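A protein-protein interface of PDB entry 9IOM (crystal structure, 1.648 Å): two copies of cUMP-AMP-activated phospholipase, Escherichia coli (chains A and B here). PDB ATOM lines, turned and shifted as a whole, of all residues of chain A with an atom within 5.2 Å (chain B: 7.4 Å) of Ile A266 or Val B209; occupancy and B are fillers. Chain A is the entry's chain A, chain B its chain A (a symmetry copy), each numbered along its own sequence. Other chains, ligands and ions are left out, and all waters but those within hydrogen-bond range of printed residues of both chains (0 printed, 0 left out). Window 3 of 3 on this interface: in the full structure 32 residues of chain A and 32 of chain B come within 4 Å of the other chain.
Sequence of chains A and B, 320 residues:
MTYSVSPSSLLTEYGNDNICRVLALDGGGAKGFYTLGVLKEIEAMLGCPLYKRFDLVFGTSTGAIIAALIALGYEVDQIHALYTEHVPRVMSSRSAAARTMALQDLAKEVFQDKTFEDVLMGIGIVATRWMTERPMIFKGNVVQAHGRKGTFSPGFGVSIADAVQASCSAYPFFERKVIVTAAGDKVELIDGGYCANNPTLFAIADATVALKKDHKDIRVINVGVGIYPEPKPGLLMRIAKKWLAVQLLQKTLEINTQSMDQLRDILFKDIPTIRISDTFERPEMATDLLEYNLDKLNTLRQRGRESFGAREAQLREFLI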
ATOM      1  N   GLN A 262     -26.585 -22.568  20.669  1.00  0.00           N
ATOM      2  CA  GLN A 262     -26.607 -22.728  19.221  1.00  0.00           C
ATOM      3  C   GLN A 262     -25.316 -22.224  18.596  1.00  0.00           C
ATOM      4  O   GLN A 262     -24.784 -22.845  17.664  1.00  0.00           O
ATOM      5  CB  GLN A 262     -27.798 -21.987  18.635  1.00  0.00           C
ATOM      6  CG  GLN A 262     -28.017 -22.277  17.165  1.00  0.00           C
ATOM      7  CD  GLN A 262     -28.462 -23.714  16.927  1.00  0.00           C
ATOM      8  OE1 GLN A 262     -29.008 -24.370  17.828  1.00  0.00           O
ATOM      9  NE2 GLN A 262     -28.229 -24.215  15.716  1.00  0.00           N
ATOM     10  N   LEU A 263     -24.800 -21.091  19.093  1.00  0.00           N
ATOM     11  CA  LEU A 263     -23.540 -20.570  18.568  1.00  0.00           C
ATOM     12  C   LEU A 263     -22.414 -21.565  18.802  1.00  0.00           C
ATOM     13  O   LEU A 263     -21.578 -21.786  17.919  1.00  0.00           O
ATOM     14  CB  LEU A 263     -23.213 -19.218  19.216  1.00  0.00           C
ATOM     15  CG  LEU A 263     -21.933 -18.507  18.740  1.00  0.00           C
ATOM     16  CD1 LEU A 263     -21.949 -18.280  17.233  1.00  0.00           C
ATOM     17  CD2 LEU A 263     -21.714 -17.178  19.481  1.00  0.00           C
ATOM     18  N   ARG A 264     -22.389 -22.187  19.983  1.00  0.00           N
ATOM     19  CA  ARG A 264     -21.415 -23.240  20.246  1.00  0.00           C
ATOM     20  C   ARG A 264     -21.516 -24.354  19.215  1.00  0.00           C
ATOM     21  O   ARG A 264     -20.499 -24.805  18.674  1.00  0.00           O
ATOM     22  CB  ARG A 264     -21.613 -23.816  21.648  1.00  0.00           C
ATOM     23  CG  ARG A 264     -20.668 -24.979  21.938  1.00  0.00           C
ATOM     24  CD  ARG A 264     -21.107 -25.797  23.146  1.00  0.00           C
ATOM     25  NE  ARG A 264     -22.477 -26.272  23.000  1.00  0.00           N
ATOM     26  CZ  ARG A 264     -22.859 -27.235  22.166  1.00  0.00           C
ATOM     27  NH1 ARG A 264     -21.970 -27.845  21.390  1.00  0.00           N
ATOM     28  NH2 ARG A 264     -24.135 -27.584  22.106  1.00  0.00           N
ATOM     29  N   ASP A 265     -22.736 -24.827  18.947  1.00  0.00           N
ATOM     30  CA  ASP A 265     -22.900 -25.942  18.018  1.00  0.00           C
ATOM     31  C   ASP A 265     -22.457 -25.560  16.612  1.00  0.00           C
ATOM     32  O   ASP A 265     -21.968 -26.410  15.862  1.00  0.00           O
ATOM     33  CB  ASP A 265     -24.350 -26.416  18.003  1.00  0.00           C
ATOM     34  CG  ASP A 265     -24.548 -27.632  17.117  1.00  0.00           C
ATOM     35  OD1 ASP A 265     -23.840 -28.647  17.333  1.00  0.00           O
ATOM     36  OD2 ASP A 265     -25.401 -27.567  16.205  1.00  0.00           O
ATOM     37  N   ILE A 266     -22.595 -24.288  16.248  1.00  0.00           N
ATOM     38  CA  ILE A 266     -22.155 -23.837  14.931  1.00  0.00           C
ATOM     39  C   ILE A 266     -20.630 -23.797  14.855  1.00  0.00           C
ATOM     40  O   ILE A 266     -20.028 -24.272  13.885  1.00  0.00           O
ATOM     41  CB  ILE A 266     -22.763 -22.461  14.616  1.00  0.00           C
ATOM     42  CG1 ILE A 266     -24.271 -22.570  14.426  1.00  0.00           C
ATOM     43  CG2 ILE A 266     -22.122 -21.881  13.385  1.00  0.00           C
ATOM     44  CD1 ILE A 266     -24.972 -21.221  14.545  1.00  0.00           C
ATOM     45  N   LEU A 267     -19.982 -23.219  15.866  1.00  0.00           N
ATOM     46  CA  LEU A 267     -18.545 -22.943  15.804  1.00  0.00           C
ATOM     47  C   LEU A 267     -17.671 -24.104  16.252  1.00  0.00           C
ATOM     48  O   LEU A 267     -16.479 -24.128  15.907  1.00  0.00           O
ATOM     49  CB  LEU A 267     -18.180 -21.742  16.681  1.00  0.00           C
ATOM     50  CG  LEU A 267     -18.789 -20.378  16.357  1.00  0.00           C
ATOM     51  CD1 LEU A 267     -18.394 -19.379  17.420  1.00  0.00           C
ATOM     52  CD2 LEU A 267     -18.348 -19.921  14.986  1.00  0.00           C
ATOM     53  N   PHE A 268     -18.205 -25.034  17.041  1.00  0.00           N
ATOM     54  CA  PHE A 268     -17.389 -26.086  17.641  1.00  0.00           C
ATOM     55  C   PHE A 268     -18.084 -27.431  17.499  1.00  0.00           C
ATOM     56  O   PHE A 268     -18.275 -28.167  18.467  1.00  0.00           O
ATOM     57  CB  PHE A 268     -17.082 -25.770  19.100  1.00  0.00           C
ATOM     58  CG  PHE A 268     -16.246 -24.550  19.267  1.00  0.00           C
ATOM     59  CD1 PHE A 268     -14.888 -24.588  18.996  1.00  0.00           C
ATOM     60  CD2 PHE A 268     -16.823 -23.352  19.655  1.00  0.00           C
ATOM     61  CE1 PHE A 268     -14.113 -23.455  19.124  1.00  0.00           C
ATOM     62  CE2 PHE A 268     -16.058 -22.218  19.781  1.00  0.00           C
ATOM     63  CZ  PHE A 268     -14.698 -22.267  19.521  1.00  0.00           C
ATOM     64  N   LYS A 269     -18.451 -27.764  16.257  1.00  0.00           N
ATOM     65  CA  LYS A 269     -19.028 -29.070  15.956  1.00  0.00           C
ATOM     66  C   LYS A 269     -18.191 -30.205  16.523  1.00  0.00           C
ATOM     67  O   LYS A 269     -18.736 -31.222  16.961  1.00  0.00           O
ATOM     68  CB  LYS A 269     -19.160 -29.233  14.444  1.00  0.00           C
ATOM     69  CG  LYS A 269     -20.428 -28.669  13.861  1.00  0.00           C
ATOM     70  CD  LYS A 269     -21.648 -29.165  14.609  1.00  0.00           C
ATOM     71  CE  LYS A 269     -22.856 -29.234  13.684  1.00  0.00           C
ATOM     72  NZ  LYS A 269     -23.691 -28.002  13.771  1.00  0.00           N
ATOM     73  N   PRO B 135     -31.240 -18.409  17.065  1.00  0.00           N
ATOM     74  CA  PRO B 135     -31.289 -17.600  15.845  1.00  0.00           C
ATOM     75  C   PRO B 135     -31.887 -18.352  14.663  1.00  0.00           C
ATOM     76  O   PRO B 135     -31.819 -19.581  14.570  1.00  0.00           O
ATOM     77  CB  PRO B 135     -29.821 -17.236  15.590  1.00  0.00           C
ATOM     78  CG  PRO B 135     -29.017 -18.156  16.443  1.00  0.00           C
ATOM     79  CD  PRO B 135     -29.874 -18.544  17.604  1.00  0.00           C
ATOM     80  N   ILE B 137     -31.318 -17.571  10.624  1.00  0.00           N
ATOM     81  CA  ILE B 137     -30.490 -16.734   9.763  1.00  0.00           C
ATOM     82  C   ILE B 137     -30.924 -16.952   8.320  1.00  0.00           C
ATOM     83  O   ILE B 137     -30.774 -18.055   7.775  1.00  0.00           O
ATOM     84  CB  ILE B 137     -29.005 -17.040   9.963  1.00  0.00           C
ATOM     85  CG1 ILE B 137     -28.670 -16.974  11.459  1.00  0.00           C
ATOM     86  CG2 ILE B 137     -28.145 -16.070   9.155  1.00  0.00           C
ATOM     87  CD1 ILE B 137     -27.210 -17.149  11.751  1.00  0.00           C
ATOM     88  N   LYS B 139     -30.314 -16.562   4.517  1.00  0.00           N
ATOM     89  CA  LYS B 139     -29.099 -16.446   3.720  1.00  0.00           C
ATOM     90  C   LYS B 139     -29.412 -16.463   2.232  1.00  0.00           C
ATOM     91  O   LYS B 139     -30.373 -17.098   1.785  1.00  0.00           O
ATOM     92  CB  LYS B 139     -28.119 -17.568   4.028  1.00  0.00           C
ATOM     93  CG  LYS B 139     -27.539 -17.490   5.419  1.00  0.00           C
ATOM     94  CD  LYS B 139     -26.745 -18.743   5.748  1.00  0.00           C
ATOM     95  CE  LYS B 139     -26.143 -18.663   7.142  1.00  0.00           C
ATOM     96  NZ  LYS B 139     -24.934 -19.519   7.253  1.00  0.00           N
ATOM     97  N   LEU B 201     -20.051 -12.811  14.715  1.00  0.00           N
ATOM     98  CA  LEU B 201     -19.645 -14.200  14.915  1.00  0.00           C
ATOM     99  C   LEU B 201     -20.402 -15.127  13.980  1.00  0.00           C
ATOM    100  O   LEU B 201     -19.845 -16.119  13.497  1.00  0.00           O
ATOM    101  CB  LEU B 201     -19.853 -14.624  16.371  1.00  0.00           C
ATOM    102  CG  LEU B 201     -18.684 -14.261  17.285  1.00  0.00           C
ATOM    103  CD1 LEU B 201     -19.007 -14.578  18.730  1.00  0.00           C
ATOM    104  CD2 LEU B 201     -17.431 -14.999  16.850  1.00  0.00           C
ATOM    105  N   PHE B 202     -21.669 -14.811  13.701  1.00  0.00           N
ATOM    106  CA  PHE B 202     -22.411 -15.609  12.736  1.00  0.00           C
ATOM    107  C   PHE B 202     -21.880 -15.398  11.323  1.00  0.00           C
ATOM    108  O   PHE B 202     -21.896 -16.331  10.510  1.00  0.00           O
ATOM    109  CB  PHE B 202     -23.902 -15.289  12.848  1.00  0.00           C
ATOM    110  CG  PHE B 202     -24.505 -15.767  14.140  1.00  0.00           C
ATOM    111  CD1 PHE B 202     -24.843 -17.103  14.303  1.00  0.00           C
ATOM    112  CD2 PHE B 202     -24.669 -14.908  15.212  1.00  0.00           C
ATOM    113  CE1 PHE B 202     -25.371 -17.563  15.505  1.00  0.00           C
ATOM    114  CE2 PHE B 202     -25.191 -15.361  16.410  1.00  0.00           C
ATOM    115  CZ  PHE B 202     -25.538 -16.684  16.558  1.00  0.00           C
ATOM    116  N   ALA B 203     -21.384 -14.194  11.016  1.00  0.00           N
ATOM    117  CA  ALA B 203     -20.738 -13.980   9.725  1.00  0.00           C
ATOM    118  C   ALA B 203     -19.427 -14.756   9.634  1.00  0.00           C
ATOM    119  O   ALA B 203     -19.125 -15.364   8.599  1.00  0.00           O
ATOM    120  CB  ALA B 203     -20.510 -12.486   9.492  1.00  0.00           C
ATOM    121  N   ILE B 204     -18.647 -14.771  10.718  1.00  0.00           N
ATOM    122  CA  ILE B 204     -17.405 -15.540  10.716  1.00  0.00           C
ATOM    123  C   ILE B 204     -17.702 -17.029  10.566  1.00  0.00           C
ATOM    124  O   ILE B 204     -16.985 -17.753   9.865  1.00  0.00           O
ATOM    125  CB  ILE B 204     -16.596 -15.245  11.993  1.00  0.00           C
ATOM    126  CG1 ILE B 204     -15.950 -13.859  11.891  1.00  0.00           C
ATOM    127  CG2 ILE B 204     -15.577 -16.366  12.259  1.00  0.00           C
ATOM    128  CD1 ILE B 204     -15.345 -13.343  13.205  1.00  0.00           C
ATOM    129  N   ALA B 205     -18.766 -17.513  11.213  1.00  0.00           N
ATOM    130  CA  ALA B 205     -19.124 -18.918  11.059  1.00  0.00           C
ATOM    131  C   ALA B 205     -19.439 -19.233   9.603  1.00  0.00           C
ATOM    132  O   ALA B 205     -19.034 -20.278   9.080  1.00  0.00           O
ATOM    133  CB  ALA B 205     -20.314 -19.258  11.958  1.00  0.00           C
ATOM    134  N   ASP B 206     -20.131 -18.315   8.926  1.00  0.00           N
ATOM    135  CA  ASP B 206     -20.463 -18.503   7.519  1.00  0.00           C
ATOM    136  C   ASP B 206     -19.206 -18.544   6.663  1.00  0.00           C
ATOM    137  O   ASP B 206     -19.082 -19.391   5.773  1.00  0.00           O
ATOM    138  CB  ASP B 206     -21.394 -17.381   7.061  1.00  0.00           C
ATOM    139  CG  ASP B 206     -22.148 -17.721   5.798  1.00  0.00           C
ATOM    140  OD1 ASP B 206     -22.869 -18.744   5.780  1.00  0.00           O
ATOM    141  OD2 ASP B 206     -22.029 -16.950   4.823  1.00  0.00           O
ATOM    142  N   ALA B 207     -18.254 -17.646   6.925  1.00  0.00           N
ATOM    143  CA  ALA B 207     -17.028 -17.615   6.134  1.00  0.00           C
ATOM    144  C   ALA B 207     -16.161 -18.846   6.390  1.00  0.00           C
ATOM    145  O   ALA B 207     -15.553 -19.387   5.458  1.00  0.00           O
ATOM    146  CB  ALA B 207     -16.252 -16.333   6.429  1.00  0.00           C
ATOM    147  N   THR B 208     -16.101 -19.319   7.637  1.00  0.00           N
ATOM    148  CA  THR B 208     -15.235 -20.447   7.972  1.00  0.00           C
ATOM    149  C   THR B 208     -15.900 -21.804   7.759  1.00  0.00           C
ATOM    150  O   THR B 208     -15.243 -22.744   7.300  1.00  0.00           O
ATOM    151  CB  THR B 208     -14.768 -20.349   9.426  1.00  0.00           C
ATOM    152  OG1 THR B 208     -15.909 -20.385  10.300  1.00  0.00           O
ATOM    153  CG2 THR B 208     -13.985 -19.067   9.641  1.00  0.00           C
ATOM    154  N   VAL B 209     -17.181 -21.937   8.091  1.00  0.00           N
ATOM    155  CA  VAL B 209     -17.826 -23.250   8.112  1.00  0.00           C
ATOM    156  C   VAL B 209     -18.513 -23.563   6.790  1.00  0.00           C
ATOM    157  O   VAL B 209     -18.534 -24.717   6.358  1.00  0.00           O
ATOM    158  CB  VAL B 209     -18.815 -23.331   9.291  1.00  0.00           C
ATOM    159  CG1 VAL B 209     -19.612 -24.628   9.244  1.00  0.00           C
ATOM    160  CG2 VAL B 209     -18.075 -23.199  10.612  1.00  0.00           C
ATOM    161  N   ALA B 210     -19.092 -22.562   6.127  1.00  0.00           N
ATOM    162  CA  ALA B 210     -19.749 -22.768   4.841  1.00  0.00           C
ATOM    163  C   ALA B 210     -18.816 -22.471   3.672  1.00  0.00           C
ATOM    164  O   ALA B 210     -18.609 -23.326   2.806  1.00  0.00           O
ATOM    165  CB  ALA B 210     -21.017 -21.910   4.747  1.00  0.00           C
ATOM    166  N   LEU B 211     -18.248 -21.267   3.629  1.00  0.00           N
ATOM    167  CA  LEU B 211     -17.332 -20.882   2.561  1.00  0.00           C
ATOM    168  C   LEU B 211     -15.939 -21.480   2.727  1.00  0.00           C
ATOM    169  O   LEU B 211     -15.082 -21.251   1.864  1.00  0.00           O
ATOM    170  CB  LEU B 211     -17.237 -19.357   2.479  1.00  0.00           C
ATOM    171  CG  LEU B 211     -18.577 -18.652   2.251  1.00  0.00           C
ATOM    172  CD1 LEU B 211     -18.441 -17.146   2.398  1.00  0.00           C
ATOM    173  CD2 LEU B 211     -19.138 -18.999   0.881  1.00  0.00           C
ATOM    174  N   LYS B 212     -15.704 -22.229   3.806  1.00  0.00           N
ATOM    175  CA  LYS B 212     -14.447 -22.943   4.059  1.00  0.00           C
ATOM    176  C   LYS B 212     -13.228 -22.073   3.770  1.00  0.00           C
ATOM    177  O   LYS B 212     -12.309 -22.464   3.049  1.00  0.00           O
ATOM    178  CB  LYS B 212     -14.375 -24.243   3.254  1.00  0.00           C
ATOM    179  CG  LYS B 212     -15.707 -24.948   3.001  1.00  0.00           C
ATOM    180  CD  LYS B 212     -16.427 -25.309   4.290  1.00  0.00           C
ATOM    181  CE  LYS B 212     -15.637 -26.276   5.167  1.00  0.00           C
ATOM    182  NZ  LYS B 212     -16.276 -26.443   6.513  1.00  0.00           N
ATOM    183  N   LYS B 213     -13.219 -20.872   4.338  1.00  0.00           N
ATOM    184  CA  LYS B 213     -12.072 -19.983   4.216  1.00  0.00           C
ATOM    185  C   LYS B 213     -11.153 -20.151   5.417  1.00  0.00           C
ATOM    186  O   LYS B 213     -11.615 -20.333   6.549  1.00  0.00           O
ATOM    187  CB  LYS B 213     -12.508 -18.521   4.097  1.00  0.00           C
ATOM    188  CG  LYS B 213     -13.259 -18.200   2.818  1.00  0.00           C
ATOM    189  CD  LYS B 213     -12.424 -18.518   1.580  1.00  0.00           C
ATOM    190  CE  LYS B 213     -11.145 -17.703   1.543  1.00  0.00           C
ATOM    191  NZ  LYS B 213     -10.395 -17.928   0.279  1.00  0.00           N
ATOM    192  N   ILE B 218      -9.406 -14.078   5.673  1.00  0.00           N
ATOM    193  CA  ILE B 218     -10.659 -13.395   5.975  1.00  0.00           C
ATOM    194  C   ILE B 218     -10.348 -11.982   6.446  1.00  0.00           C
ATOM    195  O   ILE B 218      -9.379 -11.766   7.182  1.00  0.00           O
ATOM    196  CB  ILE B 218     -11.474 -14.165   7.040  1.00  0.00           C
ATOM    197  CG1 ILE B 218     -11.772 -15.586   6.553  1.00  0.00           C
ATOM    198  CG2 ILE B 218     -12.776 -13.422   7.378  1.00  0.00           C
ATOM    199  CD1 ILE B 218     -12.409 -16.484   7.595  1.00  0.00           C
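Of the 8 printed residues of chain A, 3 touch a printed residue of chain B.
Printed residues of chain A that touch a printed residue of chain B: Leu A263, Ile A266 and Leu A267.
Hydrophobic or aromatic side chains of chain A that line the printed part of chain B: Leu A263, Ile A266 and Leu A267.
Hydrophobic or aromatic side chains of chain B that line the printed part of chain A: Leu B201, Phe B202, Ala B205 and Val B209.
Among the printed residues, 6 pairs touch across the chains.
Leu B201 touches Leu A263.
Leu A263 touches Phe B202 (CD1 to CE1, 3.9 Å).
Phe B202 touches Ile A266.
Ala B205 touches Ile A266 (CB to CG2, 3.5 Å).
Ile A266 touches Val B209 (O to CG2, 3.96 Å).
Leu A267 touches Ala B205.
Of chain B, only Phe B202, Ala B205 and Val B209 come within 4 Å of Ile A266.
Val B209 touches just one residue of chain A: Ile A266.
Printed residues of chain B within 4 Å of Leu A263: Leu B201 (3.8 Å) and Phe B202 (3.9 Å).
Of the printed residues of chain A, Phe B202 touches Leu A263 and Ile A266.
Ala B207 touches none of the printed residues of chain A.
Phe A268 touches none of the printed residues of chain B.
The nearest printed residue of chain B that does not touch Ile A266 is Pro B135 (5.4 Å).
The nearest printed residue of chain A that does not touch Ala B205 is Leu A263 (5.6 Å).
No position is printed for both chains.
The side-chain amino group of Lys B212 sits at hydrogen-bond distance from the backbone carbonyl oxygen of Val B209 (2.8 Å).
O of Ala B205 is in hydrogen-bond range of OG1 of Thr B208, at 3.4 Å.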
